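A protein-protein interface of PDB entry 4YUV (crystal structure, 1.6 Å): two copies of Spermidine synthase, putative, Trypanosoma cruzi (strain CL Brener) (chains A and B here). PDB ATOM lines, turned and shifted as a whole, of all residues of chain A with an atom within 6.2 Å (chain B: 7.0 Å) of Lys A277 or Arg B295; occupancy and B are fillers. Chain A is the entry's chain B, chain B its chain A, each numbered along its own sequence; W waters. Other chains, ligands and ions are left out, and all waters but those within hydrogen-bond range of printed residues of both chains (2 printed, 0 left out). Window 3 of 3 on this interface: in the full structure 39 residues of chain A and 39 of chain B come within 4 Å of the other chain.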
ATOM      1  N   GLU A  83       6.917 -14.280 -18.705  1.00  0.00           N
ATOM      2  CA  GLU A  83       6.887 -13.736 -20.103  1.00  0.00           C
ATOM      3  C   GLU A  83       7.279 -14.869 -21.124  1.00  0.00           C
ATOM      4  O   GLU A  83       6.654 -14.943 -22.158  1.00  0.00           O
ATOM      5  CB  GLU A  83       7.822 -12.577 -20.256  1.00  0.00           C
ATOM      6  CG  GLU A  83       7.244 -11.330 -19.584  1.00  0.00           C
ATOM      7  CD  GLU A  83       8.189 -10.186 -19.742  1.00  0.00           C
ATOM      8  OE1 GLU A  83       9.052 -10.193 -20.594  1.00  0.00           O
ATOM      9  OE2 GLU A  83       8.007  -9.149 -18.986  1.00  0.00           O
ATOM     10  N   MET A 273       2.103  -6.037 -31.533  1.00  0.00           N
ATOM     11  CA  MET A 273       1.095  -6.022 -30.468  1.00  0.00           C
ATOM     12  C   MET A 273       1.258  -4.793 -29.585  1.00  0.00           C
ATOM     13  O   MET A 273       2.353  -4.338 -29.301  1.00  0.00           O
ATOM     14  CB  MET A 273       1.178  -7.342 -29.630  1.00  0.00           C
ATOM     15  CG  MET A 273       0.961  -8.503 -30.578  1.00  0.00           C
ATOM     16  SD  MET A 273       0.939 -10.126 -29.672  1.00  0.00           S
ATOM     17  CE  MET A 273       0.925 -11.372 -30.910  1.00  0.00           C
ATOM     18  N   PRO A 274       0.141  -4.282 -29.052  1.00  0.00           N
ATOM     19  CA  PRO A 274       0.242  -3.044 -28.297  1.00  0.00           C
ATOM     20  C   PRO A 274       0.959  -3.152 -26.955  1.00  0.00           C
ATOM     21  O   PRO A 274       1.360  -2.140 -26.383  1.00  0.00           O
ATOM     22  CB  PRO A 274      -1.228  -2.589 -28.144  1.00  0.00           C
ATOM     23  CG  PRO A 274      -2.097  -3.763 -28.517  1.00  0.00           C
ATOM     24  CD  PRO A 274      -1.243  -4.792 -29.235  1.00  0.00           C
ATOM     25  N   PHE A 275       1.211  -4.387 -26.452  1.00  0.00           N
ATOM     26  CA  PHE A 275       1.786  -4.527 -25.130  1.00  0.00           C
ATOM     27  C   PHE A 275       3.293  -4.918 -25.145  1.00  0.00           C
ATOM     28  O   PHE A 275       3.903  -5.108 -24.119  1.00  0.00           O
ATOM     29  CB  PHE A 275       1.032  -5.615 -24.315  1.00  0.00           C
ATOM     30  CG  PHE A 275       1.036  -6.957 -24.987  1.00  0.00           C
ATOM     31  CD1 PHE A 275       2.081  -7.856 -24.752  1.00  0.00           C
ATOM     32  CD2 PHE A 275      -0.013  -7.367 -25.801  1.00  0.00           C
ATOM     33  CE1 PHE A 275       2.041  -9.094 -25.400  1.00  0.00           C
ATOM     34  CE2 PHE A 275      -0.021  -8.602 -26.447  1.00  0.00           C
ATOM     35  CZ  PHE A 275       1.037  -9.442 -26.222  1.00  0.00           C
ATOM     36  N   ALA A 276       3.863  -4.927 -26.358  1.00  0.00           N
ATOM     37  CA  ALA A 276       5.283  -5.333 -26.521  1.00  0.00           C
ATOM     38  C   ALA A 276       6.164  -4.504 -25.650  1.00  0.00           C
ATOM     39  O   ALA A 276       7.020  -4.994 -24.914  1.00  0.00           O
ATOM     40  CB  ALA A 276       5.710  -5.290 -27.988  1.00  0.00           C
ATOM     41  N   LYS A 277       5.875  -3.196 -25.594  1.00  0.00           N
ATOM     42  CA  LYS A 277       6.730  -2.324 -24.807  1.00  0.00           C
ATOM     43  C   LYS A 277       6.581  -2.451 -23.308  1.00  0.00           C
ATOM     44  O   LYS A 277       7.342  -1.820 -22.560  1.00  0.00           O
ATOM     45  CB  LYS A 277       6.303  -0.867 -25.140  1.00  0.00           C
ATOM     46  CG  LYS A 277       6.476  -0.482 -26.608  1.00  0.00           C
ATOM     47  CD  LYS A 277       7.954  -0.482 -26.986  1.00  0.00           C
ATOM     48  CE  LYS A 277       8.170   0.111 -28.373  1.00  0.00           C
ATOM     49  NZ  LYS A 277       9.164  -0.673 -29.171  1.00  0.00           N
ATOM     50  N   ASP A 278       5.579  -3.170 -22.829  1.00  0.00           N
ATOM     51  CA  ASP A 278       5.384  -3.401 -21.430  1.00  0.00           C
ATOM     52  C   ASP A 278       6.226  -4.550 -20.901  1.00  0.00           C
ATOM     53  O   ASP A 278       6.336  -4.694 -19.674  1.00  0.00           O
ATOM     54  CB  ASP A 278       3.917  -3.729 -21.041  1.00  0.00           C
ATOM     55  CG  ASP A 278       2.873  -2.686 -21.507  1.00  0.00           C
ATOM     56  OD1 ASP A 278       3.217  -1.512 -21.531  1.00  0.00           O
ATOM     57  OD2 ASP A 278       1.733  -3.084 -21.904  1.00  0.00           O
ATOM     58  N   LEU A 279       6.788  -5.345 -21.832  1.00  0.00           N
ATOM     59  CA  LEU A 279       7.517  -6.536 -21.350  1.00  0.00           C
ATOM     60  C   LEU A 279       8.946  -6.202 -20.892  1.00  0.00           C
ATOM     61  O   LEU A 279       9.576  -5.323 -21.495  1.00  0.00           O
ATOM     62  CB  LEU A 279       7.522  -7.555 -22.496  1.00  0.00           C
ATOM     63  CG  LEU A 279       6.125  -7.975 -23.012  1.00  0.00           C
ATOM     64  CD1 LEU A 279       6.269  -9.078 -24.024  1.00  0.00           C
ATOM     65  CD2 LEU A 279       5.147  -8.301 -21.880  1.00  0.00           C
ATOM     66  N   LYS A 280       9.455  -6.907 -19.876  1.00  0.00           N
ATOM     67  CA  LYS A 280      10.804  -6.689 -19.294  1.00  0.00           C
ATOM     68  C   LYS A 280      11.857  -7.619 -19.825  1.00  0.00           C
ATOM     69  O   LYS A 280      13.057  -7.273 -19.756  1.00  0.00           O
ATOM     70  CB  LYS A 280      10.744  -6.741 -17.777  1.00  0.00           C
ATOM     71  CG  LYS A 280       9.990  -5.530 -17.152  1.00  0.00           C
ATOM     72  CD  LYS A 280       9.664  -5.801 -15.671  1.00  0.00           C
ATOM     73  CE  LYS A 280       9.036  -4.546 -15.047  1.00  0.00           C
ATOM     74  NZ  LYS A 280       7.607  -4.438 -15.514  1.00  0.00           N
ATOM     75  N   TYR A 281      11.488  -8.759 -20.453  1.00  0.00           N
ATOM     76  CA  TYR A 281      12.461  -9.730 -20.959  1.00  0.00           C
ATOM     77  C   TYR A 281      12.225 -10.119 -22.398  1.00  0.00           C
ATOM     78  O   TYR A 281      13.012  -9.957 -23.290  1.00  0.00           O
ATOM     79  CB  TYR A 281      12.355 -10.989 -20.048  1.00  0.00           C
ATOM     80  CG  TYR A 281      13.339 -12.113 -20.384  1.00  0.00           C
ATOM     81  CD1 TYR A 281      13.045 -13.072 -21.376  1.00  0.00           C
ATOM     82  CD2 TYR A 281      14.624 -12.159 -19.695  1.00  0.00           C
ATOM     83  CE1 TYR A 281      13.991 -14.089 -21.638  1.00  0.00           C
ATOM     84  CE2 TYR A 281      15.517 -13.218 -20.000  1.00  0.00           C
ATOM     85  CZ  TYR A 281      15.186 -14.099 -20.967  1.00  0.00           C
ATOM     86  OH  TYR A 281      16.081 -15.143 -21.163  1.00  0.00           O
ATOM     87  N   TYR A 282      11.040 -10.590 -22.685  1.00  0.00           N
ATOM     88  CA  TYR A 282      10.719 -11.114 -23.999  1.00  0.00           C
ATOM     89  C   TYR A 282      10.518 -10.169 -25.136  1.00  0.00           C
ATOM     90  O   TYR A 282       9.874  -9.119 -24.948  1.00  0.00           O
ATOM     91  CB  TYR A 282       9.443 -12.027 -23.834  1.00  0.00           C
ATOM     92  CG  TYR A 282       8.918 -12.645 -25.083  1.00  0.00           C
ATOM     93  CD1 TYR A 282       8.142 -11.964 -26.016  1.00  0.00           C
ATOM     94  CD2 TYR A 282       9.323 -13.994 -25.467  1.00  0.00           C
ATOM     95  CE1 TYR A 282       7.675 -12.523 -27.169  1.00  0.00           C
ATOM     96  CE2 TYR A 282       8.882 -14.565 -26.621  1.00  0.00           C
ATOM     97  CZ  TYR A 282       8.085 -13.871 -27.528  1.00  0.00           C
ATOM     98  OH  TYR A 282       7.604 -14.360 -28.665  1.00  0.00           O
ATOM     99  N   ASP A 283      11.092 -10.532 -26.290  1.00  0.00           N
ATOM    100  CA  ASP A 283      10.769  -9.931 -27.589  1.00  0.00           C
ATOM    101  C   ASP A 283      11.101 -10.924 -28.654  1.00  0.00           C
ATOM    102  O   ASP A 283      11.519 -12.043 -28.326  1.00  0.00           O
ATOM    103  CB  ASP A 283      11.451  -8.558 -27.751  1.00  0.00           C
ATOM    104  CG  ASP A 283      12.974  -8.630 -27.838  1.00  0.00           C
ATOM    105  OD1 ASP A 283      13.567  -9.684 -28.076  1.00  0.00           O
ATOM    106  OD2 ASP A 283      13.577  -7.539 -27.545  1.00  0.00           O
ATOM    107  N   MET A 286      14.671 -12.251 -28.621  1.00  0.00           N
ATOM    108  CA  MET A 286      14.930 -13.153 -27.473  1.00  0.00           C
ATOM    109  C   MET A 286      14.207 -14.490 -27.752  1.00  0.00           C
ATOM    110  O   MET A 286      14.774 -15.553 -27.414  1.00  0.00           O
ATOM    111  CB  MET A 286      14.490 -12.549 -26.129  1.00  0.00           C
ATOM    112  CG  MET A 286      15.408 -11.401 -25.638  1.00  0.00           C
ATOM    113  SD  MET A 286      17.015 -12.146 -25.243  1.00  0.00           S
ATOM    114  CE  MET A 286      16.621 -12.929 -23.707  1.00  0.00           C
ATOM    115  N   LEU B 293      19.571  -9.613 -26.156  1.00  0.00           N
ATOM    116  CA  LEU B 293      19.548  -9.382 -24.702  1.00  0.00           C
ATOM    117  C   LEU B 293      18.095  -9.208 -24.215  1.00  0.00           C
ATOM    118  O   LEU B 293      17.284  -8.648 -24.983  1.00  0.00           O
ATOM    119  CB  LEU B 293      20.339  -8.086 -24.266  1.00  0.00           C
ATOM    120  CG  LEU B 293      21.774  -8.063 -24.768  1.00  0.00           C
ATOM    121  CD1 LEU B 293      22.483  -6.731 -24.328  1.00  0.00           C
ATOM    122  CD2 LEU B 293      22.521  -9.294 -24.278  1.00  0.00           C
ATOM    123  N   PRO B 294      17.859  -9.555 -22.939  1.00  0.00           N
ATOM    124  CA  PRO B 294      16.538  -9.254 -22.353  1.00  0.00           C
ATOM    125  C   PRO B 294      16.111  -7.783 -22.617  1.00  0.00           C
ATOM    126  O   PRO B 294      16.958  -6.872 -22.680  1.00  0.00           O
ATOM    127  CB  PRO B 294      16.816  -9.415 -20.868  1.00  0.00           C
ATOM    128  CG  PRO B 294      17.810 -10.565 -20.813  1.00  0.00           C
ATOM    129  CD  PRO B 294      18.754 -10.200 -21.965  1.00  0.00           C
ATOM    130  N   ARG B 295      14.837  -7.552 -22.818  1.00  0.00           N
ATOM    131  CA  ARG B 295      14.396  -6.166 -23.095  1.00  0.00           C
ATOM    132  C   ARG B 295      14.981  -5.126 -22.146  1.00  0.00           C
ATOM    133  O   ARG B 295      15.389  -4.033 -22.606  1.00  0.00           O
ATOM    134  CB  ARG B 295      12.852  -6.137 -23.043  1.00  0.00           C
ATOM    135  CG  ARG B 295      12.343  -6.134 -24.426  1.00  0.00           C
ATOM    136  CD  ARG B 295      10.872  -5.836 -24.630  1.00  0.00           C
ATOM    137  NE  ARG B 295      10.446  -4.700 -23.828  1.00  0.00           N
ATOM    138  CZ  ARG B 295      10.510  -3.469 -24.269  1.00  0.00           C
ATOM    139  NH1 ARG B 295      11.029  -3.247 -25.441  1.00  0.00           N
ATOM    140  NH2 ARG B 295      10.120  -2.491 -23.496  1.00  0.00           N
ATOM    141  N   PHE B 296      15.013  -5.403 -20.852  1.00  0.00           N
ATOM    142  CA  PHE B 296      15.557  -4.443 -19.830  1.00  0.00           C
ATOM    143  C   PHE B 296      17.001  -4.036 -20.116  1.00  0.00           C
ATOM    144  O   PHE B 296      17.425  -2.965 -19.681  1.00  0.00           O
ATOM    145  CB  PHE B 296      15.341  -4.950 -18.413  1.00  0.00           C
ATOM    146  CG  PHE B 296      16.249  -6.092 -17.977  1.00  0.00           C
ATOM    147  CD1 PHE B 296      17.565  -5.801 -17.539  1.00  0.00           C
ATOM    148  CD2 PHE B 296      15.794  -7.435 -17.917  1.00  0.00           C
ATOM    149  CE1 PHE B 296      18.364  -6.766 -17.023  1.00  0.00           C
ATOM    150  CE2 PHE B 296      16.620  -8.383 -17.488  1.00  0.00           C
ATOM    151  CZ  PHE B 296      17.920  -8.081 -17.061  1.00  0.00           C
ATOM    152  N   ALA B 297      17.764  -4.911 -20.800  1.00  0.00           N
ATOM    153  CA  ALA B 297      19.171  -4.659 -21.125  1.00  0.00           C
ATOM    154  C   ALA B 297      19.449  -4.333 -22.556  1.00  0.00           C
ATOM    155  O   ALA B 297      20.565  -3.997 -22.912  1.00  0.00           O
ATOM    156  CB  ALA B 297      20.018  -5.878 -20.605  1.00  0.00           C
ATOM    157  N   ARG B 298      18.480  -4.447 -23.464  1.00  0.00           N
ATOM    158  CA  ARG B 298      18.755  -4.474 -24.896  1.00  0.00           C
ATOM    159  C   ARG B 298      19.388  -3.160 -25.420  1.00  0.00           C
ATOM    160  O   ARG B 298      20.031  -3.204 -26.424  1.00  0.00           O
ATOM    161  CB  ARG B 298      17.518  -4.873 -25.709  1.00  0.00           C
ATOM    162  CG  ARG B 298      16.635  -3.793 -26.242  1.00  0.00           C
ATOM    163  CD  ARG B 298      15.702  -4.429 -27.277  1.00  0.00           C
ATOM    164  NE  ARG B 298      14.528  -3.604 -27.610  1.00  0.00           N
ATOM    165  CZ  ARG B 298      13.949  -2.672 -26.839  1.00  0.00           C
ATOM    166  NH1 ARG B 298      14.396  -2.381 -25.612  1.00  0.00           N
ATOM    167  NH2 ARG B 298      12.874  -2.032 -27.307  1.00  0.00           N
ATOM    168  N   HIS B 299      19.164  -2.062 -24.688  1.00  0.00           N
ATOM    169  CA  HIS B 299      19.688  -0.774 -25.117  1.00  0.00           C
ATOM    170  C   HIS B 299      21.202  -0.775 -25.161  1.00  0.00           C
ATOM    171  O   HIS B 299      21.751   0.022 -25.916  1.00  0.00           O
ATOM    172  CB  HIS B 299      19.233   0.372 -24.166  1.00  0.00           C
ATOM    173  CG  HIS B 299      19.565   0.112 -22.732  1.00  0.00           C
ATOM    174  ND1 HIS B 299      18.793  -0.711 -21.921  1.00  0.00           N
ATOM    175  CD2 HIS B 299      20.578   0.549 -21.947  1.00  0.00           C
ATOM    176  CE1 HIS B 299      19.315  -0.715 -20.711  1.00  0.00           C
ATOM    177  NE2 HIS B 299      20.394   0.051 -20.711  1.00  0.00           N
HETATM  178  O   HOH W   1      16.262  -8.303 -27.428  1.00  0.00           O
HETATM  179  O   HOH W   2      12.245  -5.191 -27.879  1.00  0.00           O
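The backbone NH (N) of Leu B293 sits close to the side-chain sulfur (SD) of Met A286, 3.7 Å away.
O of Lys A277 lies within hydrogen-bond range of NH2 of Arg B295 (3.0 Å).
The guanidinium group of Arg B295 is in hydrogen-bond range of the backbone carbonyl oxygen of Leu A279, 2.6 Å away.
The backbone NH (N) of Arg B295 lies within hydrogen-bond range of the backbone carbonyl oxygen (O) of Tyr A281.
N of Phe B296 sits at hydrogen-bond distance from O of Lys A280 (2.9 Å).
The side-chain sulfur (SD) of Met A286 sits close to the backbone nitrogen (N) of Pro B294 (3.6 Å).
O of Phe B296 lies close to ND1 of His B299 (3.5 Å).
The side-chain carboxylate (OE2) of Glu A83 lies within hydrogen-bond range of the backbone NH (N) of Lys A280 (2.8 Å).
OE1 of Glu A83 lies within hydrogen-bond range of N of Tyr A281 (2.8 Å).
OE1 of Glu A83 lies within hydrogen-bond range of N of Tyr A282 (2.9 Å).
The side-chain carboxylate (OD1) of Asp A283 sits at hydrogen-bond distance from the backbone NH (N) of Met A286.
Ala A276 touches Arg B295 (O to NE, 3.6 Å).
Lys A280 touches Arg B295.
Tyr A281 touches Pro B294.
Arg B295 touches Tyr A282 (CD to O, 3.4 Å).
Arg B295 touches Asp A283 (CG to OD2, 3.6 Å).
Asp A283 touches Arg B298 (OD2 to CD, 3.8 Å).
Lys A277 touches just one residue of chain B: Arg B295 (3.0 Å).
Printed residues of chain B within 4 Å of Tyr A281: Pro B294 and Arg B295.
Printed residues of chain B within 4 Å of Asp A283: Arg B295 (3.6 Å) and Arg B298 (3.8 Å).
Of the printed residues of chain A, Pro B294 touches Tyr A281 (3.6 Å) and Met A286 (3.6 Å).
Printed residues of chain B within 4 Å of Ala A276: Arg B295 (3.6 Å).
His B299 touches none of the printed residues of chain A.
Met A273 touches none of the printed residues of chain B.
The nearest residue of chain B that does not touch Lys A277 is Arg B298 (4.4 Å).
The nearest residue of chain A that does not touch Arg B295 is Asp A278 (4.6 Å).
Among the printed residues, no Asp or Glu carboxylate lies within 4 Å of a Lys or Arg side-chain nitrogen of the other chain.
No position is printed for both chains.
Water W1 bridges the backbone carbonyl oxygen of Leu B293 (2.7 Å) and the side-chain carboxylate of Asp A283 (2.8 Å).
Water W2 lies within hydrogen-bond range of the side-chain carboxylate (OD2) of Asp A283 (2.7 Å), the guanidinium group (NE) of Arg B298 (2.8 Å) and the guanidinium group (NH1) of Arg B295 (3.3 Å).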
